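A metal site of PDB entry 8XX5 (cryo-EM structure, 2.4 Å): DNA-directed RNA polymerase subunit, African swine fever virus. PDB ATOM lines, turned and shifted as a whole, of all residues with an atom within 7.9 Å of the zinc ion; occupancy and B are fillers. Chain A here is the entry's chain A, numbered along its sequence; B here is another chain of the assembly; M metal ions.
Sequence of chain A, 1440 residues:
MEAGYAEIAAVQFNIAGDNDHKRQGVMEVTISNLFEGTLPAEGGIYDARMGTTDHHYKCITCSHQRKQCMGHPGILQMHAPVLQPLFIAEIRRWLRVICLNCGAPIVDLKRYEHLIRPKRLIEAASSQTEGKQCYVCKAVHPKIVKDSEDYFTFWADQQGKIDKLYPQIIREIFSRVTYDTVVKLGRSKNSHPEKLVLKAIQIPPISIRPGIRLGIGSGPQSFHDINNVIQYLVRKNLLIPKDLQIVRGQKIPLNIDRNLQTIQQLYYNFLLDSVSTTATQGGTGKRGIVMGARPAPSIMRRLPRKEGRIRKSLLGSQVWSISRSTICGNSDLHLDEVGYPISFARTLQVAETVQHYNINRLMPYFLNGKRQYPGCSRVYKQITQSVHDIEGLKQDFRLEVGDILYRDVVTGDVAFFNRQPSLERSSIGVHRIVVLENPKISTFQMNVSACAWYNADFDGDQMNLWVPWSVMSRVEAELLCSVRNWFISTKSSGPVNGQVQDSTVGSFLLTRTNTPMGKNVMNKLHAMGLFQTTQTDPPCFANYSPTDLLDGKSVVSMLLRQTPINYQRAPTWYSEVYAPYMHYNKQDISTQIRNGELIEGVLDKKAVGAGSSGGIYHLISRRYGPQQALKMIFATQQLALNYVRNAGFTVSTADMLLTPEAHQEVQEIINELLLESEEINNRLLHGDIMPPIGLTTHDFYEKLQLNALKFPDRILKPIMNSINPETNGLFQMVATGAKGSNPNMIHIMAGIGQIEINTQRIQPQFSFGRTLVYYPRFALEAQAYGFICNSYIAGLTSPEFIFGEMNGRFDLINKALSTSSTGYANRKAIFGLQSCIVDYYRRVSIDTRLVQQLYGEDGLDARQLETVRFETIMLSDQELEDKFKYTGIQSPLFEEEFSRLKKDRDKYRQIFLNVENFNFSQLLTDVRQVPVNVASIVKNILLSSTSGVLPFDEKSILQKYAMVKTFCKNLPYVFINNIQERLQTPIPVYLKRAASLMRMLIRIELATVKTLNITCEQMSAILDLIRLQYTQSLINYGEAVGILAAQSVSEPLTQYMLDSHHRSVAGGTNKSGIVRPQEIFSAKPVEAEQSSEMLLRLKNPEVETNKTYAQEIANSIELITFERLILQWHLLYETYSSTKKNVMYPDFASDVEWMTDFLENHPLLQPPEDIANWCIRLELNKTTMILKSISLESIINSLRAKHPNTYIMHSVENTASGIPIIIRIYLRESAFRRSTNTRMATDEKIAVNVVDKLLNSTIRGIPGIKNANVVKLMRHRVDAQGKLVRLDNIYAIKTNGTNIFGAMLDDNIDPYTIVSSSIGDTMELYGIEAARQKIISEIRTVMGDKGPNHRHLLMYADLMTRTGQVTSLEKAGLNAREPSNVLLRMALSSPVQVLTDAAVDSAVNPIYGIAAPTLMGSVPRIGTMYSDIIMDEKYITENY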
ATOM      1  N   ILE A  98     -13.243  13.121  -1.513  1.00  0.00           N
ATOM      2  CA  ILE A  98     -14.405  13.298  -0.654  1.00  0.00           C
ATOM      3  C   ILE A  98     -15.483  12.292  -1.066  1.00  0.00           C
ATOM      4  O   ILE A  98     -15.575  11.910  -2.229  1.00  0.00           O
ATOM      5  CB  ILE A  98     -14.944  14.748  -0.688  1.00  0.00           C
ATOM      6  CG1 ILE A  98     -15.711  15.038  -1.985  1.00  0.00           C
ATOM      7  CG2 ILE A  98     -13.825  15.754  -0.482  1.00  0.00           C
ATOM      8  CD1 ILE A  98     -17.206  15.017  -1.801  1.00  0.00           C
ATOM      9  N   CYS A  99     -16.278  11.867  -0.087  1.00  0.00           N
ATOM     10  CA  CYS A  99     -17.312  10.865  -0.334  1.00  0.00           C
ATOM     11  C   CYS A  99     -18.451  11.467  -1.151  1.00  0.00           C
ATOM     12  O   CYS A  99     -18.979  12.532  -0.810  1.00  0.00           O
ATOM     13  CB  CYS A  99     -17.838  10.320   0.993  1.00  0.00           C
ATOM     14  SG  CYS A  99     -19.401   9.443   0.861  1.00  0.00           S
ATOM     15  N   LEU A 100     -18.836  10.777  -2.220  1.00  0.00           N
ATOM     16  CA  LEU A 100     -19.857  11.263  -3.136  1.00  0.00           C
ATOM     17  C   LEU A 100     -21.275  11.119  -2.597  1.00  0.00           C
ATOM     18  O   LEU A 100     -22.229  11.401  -3.310  1.00  0.00           O
ATOM     19  CB  LEU A 100     -19.750  10.545  -4.479  1.00  0.00           C
ATOM     20  CG  LEU A 100     -18.369  10.420  -5.125  1.00  0.00           C
ATOM     21  CD1 LEU A 100     -18.513   9.995  -6.575  1.00  0.00           C
ATOM     22  CD2 LEU A 100     -17.585  11.714  -5.035  1.00  0.00           C
ATOM     23  N   ASN A 101     -21.429  10.674  -1.342  1.00  0.00           N
ATOM     24  CA  ASN A 101     -22.738  10.479  -0.733  1.00  0.00           C
ATOM     25  C   ASN A 101     -23.041  11.518   0.340  1.00  0.00           C
ATOM     26  O   ASN A 101     -24.118  12.116   0.331  1.00  0.00           O
ATOM     27  CB  ASN A 101     -22.842   9.068  -0.142  1.00  0.00           C
ATOM     28  CG  ASN A 101     -24.271   8.607   0.022  1.00  0.00           C
ATOM     29  OD1 ASN A 101     -24.810   8.582   1.131  1.00  0.00           O
ATOM     30  ND2 ASN A 101     -24.894   8.248  -1.092  1.00  0.00           N
ATOM     31  N   CYS A 102     -22.119  11.734   1.275  1.00  0.00           N
ATOM     32  CA  CYS A 102     -22.320  12.702   2.346  1.00  0.00           C
ATOM     33  C   CYS A 102     -21.329  13.863   2.297  1.00  0.00           C
ATOM     34  O   CYS A 102     -21.448  14.782   3.122  1.00  0.00           O
ATOM     35  CB  CYS A 102     -22.224  12.005   3.704  1.00  0.00           C
ATOM     36  SG  CYS A 102     -20.644  11.209   4.028  1.00  0.00           S
ATOM     37  N   GLY A 103     -20.373  13.849   1.380  1.00  0.00           N
ATOM     38  CA  GLY A 103     -19.412  14.922   1.257  1.00  0.00           C
ATOM     39  C   GLY A 103     -18.248  14.868   2.233  1.00  0.00           C
ATOM     40  O   GLY A 103     -17.393  15.759   2.187  1.00  0.00           O
ATOM     41  N   ALA A 104     -18.192  13.867   3.095  1.00  0.00           N
ATOM     42  CA  ALA A 104     -17.080  13.751   4.021  1.00  0.00           C
ATOM     43  C   ALA A 104     -15.812  13.330   3.262  1.00  0.00           C
ATOM     44  O   ALA A 104     -15.893  12.673   2.221  1.00  0.00           O
ATOM     45  CB  ALA A 104     -17.399  12.734   5.115  1.00  0.00           C
ATOM     46  N   PRO A 105     -14.637  13.706   3.764  1.00  0.00           N
ATOM     47  CA  PRO A 105     -13.389  13.302   3.103  1.00  0.00           C
ATOM     48  C   PRO A 105     -13.096  11.830   3.348  1.00  0.00           C
ATOM     49  O   PRO A 105     -13.012  11.388   4.493  1.00  0.00           O
ATOM     50  CB  PRO A 105     -12.333  14.212   3.742  1.00  0.00           C
ATOM     51  CG  PRO A 105     -12.902  14.542   5.081  1.00  0.00           C
ATOM     52  CD  PRO A 105     -14.396  14.609   4.901  1.00  0.00           C
ATOM     53  N   ILE A 106     -12.955  11.067   2.262  1.00  0.00           N
ATOM     54  CA  ILE A 106     -12.609   9.655   2.382  1.00  0.00           C
ATOM     55  C   ILE A 106     -11.178   9.471   2.852  1.00  0.00           C
ATOM     56  O   ILE A 106     -10.850   8.424   3.421  1.00  0.00           O
ATOM     57  CB  ILE A 106     -12.843   8.922   1.052  1.00  0.00           C
ATOM     58  CG1 ILE A 106     -11.871   9.444  -0.015  1.00  0.00           C
ATOM     59  CG2 ILE A 106     -14.286   9.068   0.602  1.00  0.00           C
ATOM     60  CD1 ILE A 106     -12.282   9.112  -1.420  1.00  0.00           C
ATOM     61  N   GLN A 133     -14.114   2.783   2.111  1.00  0.00           N
ATOM     62  CA  GLN A 133     -15.409   2.830   2.771  1.00  0.00           C
ATOM     63  C   GLN A 133     -15.487   4.098   3.617  1.00  0.00           C
ATOM     64  O   GLN A 133     -14.586   4.368   4.430  1.00  0.00           O
ATOM     65  CB  GLN A 133     -15.624   1.598   3.654  1.00  0.00           C
ATOM     66  CG  GLN A 133     -17.088   1.266   3.895  1.00  0.00           C
ATOM     67  CD  GLN A 133     -17.326   0.604   5.235  1.00  0.00           C
ATOM     68  OE1 GLN A 133     -17.489  -0.617   5.318  1.00  0.00           O
ATOM     69  NE2 GLN A 133     -17.339   1.402   6.298  1.00  0.00           N
ATOM     70  N   CYS A 134     -16.546   4.864   3.417  1.00  0.00           N
ATOM     71  CA  CYS A 134     -16.779   6.050   4.231  1.00  0.00           C
ATOM     72  C   CYS A 134     -17.063   5.652   5.668  1.00  0.00           C
ATOM     73  O   CYS A 134     -17.767   4.672   5.929  1.00  0.00           O
ATOM     74  CB  CYS A 134     -17.939   6.863   3.665  1.00  0.00           C
ATOM     75  SG  CYS A 134     -18.132   8.508   4.381  1.00  0.00           S
ATOM     76  N   TYR A 135     -16.508   6.410   6.609  1.00  0.00           N
ATOM     77  CA  TYR A 135     -16.739   6.144   8.021  1.00  0.00           C
ATOM     78  C   TYR A 135     -17.957   6.878   8.568  1.00  0.00           C
ATOM     79  O   TYR A 135     -18.242   6.763   9.762  1.00  0.00           O
ATOM     80  CB  TYR A 135     -15.489   6.498   8.840  1.00  0.00           C
ATOM     81  CG  TYR A 135     -15.463   7.916   9.382  1.00  0.00           C
ATOM     82  CD1 TYR A 135     -15.336   9.003   8.528  1.00  0.00           C
ATOM     83  CD2 TYR A 135     -15.530   8.158  10.742  1.00  0.00           C
ATOM     84  CE1 TYR A 135     -15.300  10.295   9.018  1.00  0.00           C
ATOM     85  CE2 TYR A 135     -15.499   9.441  11.242  1.00  0.00           C
ATOM     86  CZ  TYR A 135     -15.385  10.510  10.385  1.00  0.00           C
ATOM     87  OH  TYR A 135     -15.342  11.791  10.878  1.00  0.00           O
ATOM     88  N   VAL A 136     -18.689   7.604   7.727  1.00  0.00           N
ATOM     89  CA  VAL A 136     -19.887   8.322   8.135  1.00  0.00           C
ATOM     90  C   VAL A 136     -21.115   7.580   7.642  1.00  0.00           C
ATOM     91  O   VAL A 136     -22.004   7.223   8.421  1.00  0.00           O
ATOM     92  CB  VAL A 136     -19.881   9.773   7.632  1.00  0.00           C
ATOM     93  CG1 VAL A 136     -21.184  10.471   7.986  1.00  0.00           C
ATOM     94  CG2 VAL A 136     -18.691  10.524   8.198  1.00  0.00           C
ATOM     95  N   CYS A 137     -21.176   7.333   6.335  1.00  0.00           N
ATOM     96  CA  CYS A 137     -22.336   6.718   5.707  1.00  0.00           C
ATOM     97  C   CYS A 137     -22.062   5.314   5.192  1.00  0.00           C
ATOM     98  O   CYS A 137     -22.968   4.701   4.603  1.00  0.00           O
ATOM     99  CB  CYS A 137     -22.846   7.601   4.559  1.00  0.00           C
ATOM    100  SG  CYS A 137     -21.729   7.673   3.141  1.00  0.00           S
ATOM    101  N   LYS A 138     -20.848   4.792   5.384  1.00  0.00           N
ATOM    102  CA  LYS A 138     -20.505   3.406   5.029  1.00  0.00           C
ATOM    103  C   LYS A 138     -20.671   3.138   3.534  1.00  0.00           C
ATOM    104  O   LYS A 138     -20.999   2.015   3.130  1.00  0.00           O
ATOM    105  CB  LYS A 138     -21.320   2.403   5.851  1.00  0.00           C
ATOM    106  CG  LYS A 138     -20.753   2.113   7.235  1.00  0.00           C
ATOM    107  CD  LYS A 138     -21.086   3.219   8.226  1.00  0.00           C
ATOM    108  CE  LYS A 138     -22.588   3.473   8.270  1.00  0.00           C
ATOM    109  NZ  LYS A 138     -22.971   4.295   9.450  1.00  0.00           N
ATOM    110  N   ALA A 139     -20.451   4.145   2.705  1.00  0.00           N
ATOM    111  CA  ALA A 139     -20.529   3.972   1.267  1.00  0.00           C
ATOM    112  C   ALA A 139     -19.151   3.685   0.681  1.00  0.00           C
ATOM    113  O   ALA A 139     -18.120   3.989   1.286  1.00  0.00           O
ATOM    114  CB  ALA A 139     -21.126   5.224   0.592  1.00  0.00           C
ATOM    115  N   VAL A 140     -19.144   3.080  -0.508  1.00  0.00           N
ATOM    116  CA  VAL A 140     -17.921   2.690  -1.186  1.00  0.00           C
ATOM    117  C   VAL A 140     -17.596   3.736  -2.239  1.00  0.00           C
ATOM    118  O   VAL A 140     -18.427   4.022  -3.109  1.00  0.00           O
ATOM    119  CB  VAL A 140     -18.048   1.291  -1.815  1.00  0.00           C
ATOM    120  CG1 VAL A 140     -16.879   1.011  -2.739  1.00  0.00           C
ATOM    121  CG2 VAL A 140     -18.143   0.231  -0.728  1.00  0.00           C
ATOM    122  N   ARG A 176     -21.752  19.349  -0.440  1.00  0.00           N
ATOM    123  CA  ARG A 176     -21.709  18.671   0.854  1.00  0.00           C
ATOM    124  C   ARG A 176     -20.349  18.748   1.519  1.00  0.00           C
ATOM    125  O   ARG A 176     -20.187  18.228   2.625  1.00  0.00           O
ATOM    126  CB  ARG A 176     -22.130  17.203   0.684  1.00  0.00           C
ATOM    127  CG  ARG A 176     -23.620  17.024   0.468  1.00  0.00           C
ATOM    128  CD  ARG A 176     -23.997  15.559   0.421  1.00  0.00           C
ATOM    129  NE  ARG A 176     -23.591  14.925  -0.836  1.00  0.00           N
ATOM    130  CZ  ARG A 176     -24.427  14.610  -1.817  1.00  0.00           C
ATOM    131  NH1 ARG A 176     -25.722  14.845  -1.734  1.00  0.00           N
ATOM    132  NH2 ARG A 176     -23.938  14.024  -2.904  1.00  0.00           N
ATOM    133  N   LEU B  51     -20.930  17.852   9.056  1.00  0.00           N
ATOM    134  CA  LEU B  51     -21.199  17.635   7.637  1.00  0.00           C
ATOM    135  C   LEU B  51     -21.912  18.849   7.061  1.00  0.00           C
ATOM    136  O   LEU B  51     -22.274  19.784   7.777  1.00  0.00           O
ATOM    137  CB  LEU B  51     -22.050  16.373   7.417  1.00  0.00           C
ATOM    138  CG  LEU B  51     -21.483  15.033   7.893  1.00  0.00           C
ATOM    139  CD1 LEU B  51     -22.094  14.637   9.213  1.00  0.00           C
ATOM    140  CD2 LEU B  51     -21.714  13.967   6.840  1.00  0.00           C
HETATM  141 ZN    ZN M   1     -19.961   9.190   3.110  1.00  0.00          ZN
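SG of Cys 102 lies close to N of Ala 104. The side-chain sulfur of Cys 137 sits close to the backbone NH of Ala 139 (3.8 Å). N of Val 136 sits close to SG of Cys 134 (3.5 Å). OD1 of Asn 101 lies close to SG of Cys 137. The backbone carbonyl oxygen of Ala 104 sits at hydrogen-bond distance from the backbone NH of Cys 99 (2.5 Å). The backbone carbonyl oxygen (O) of Ala 139 is in hydrogen-bond range of the backbone NH (N) of Cys 134 (2.8 Å). The side-chain sulfur of Cys 99 lies close to the backbone NH of Asn 101 (3.2 Å).
Within 4 Å of the zinc ion: Cys 99, Cys 102, Cys 134 and Cys 137.
The side-chain sulfur (SG) of Cys 102 binds the zinc ion. The zinc ion is bound by SG of Cys 134. The zinc ion is bound by SG of Cys 137. The zinc ion is bound by the side-chain sulfur (SG) of Cys 99. The zinc ion has four donor atoms within binding distance.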
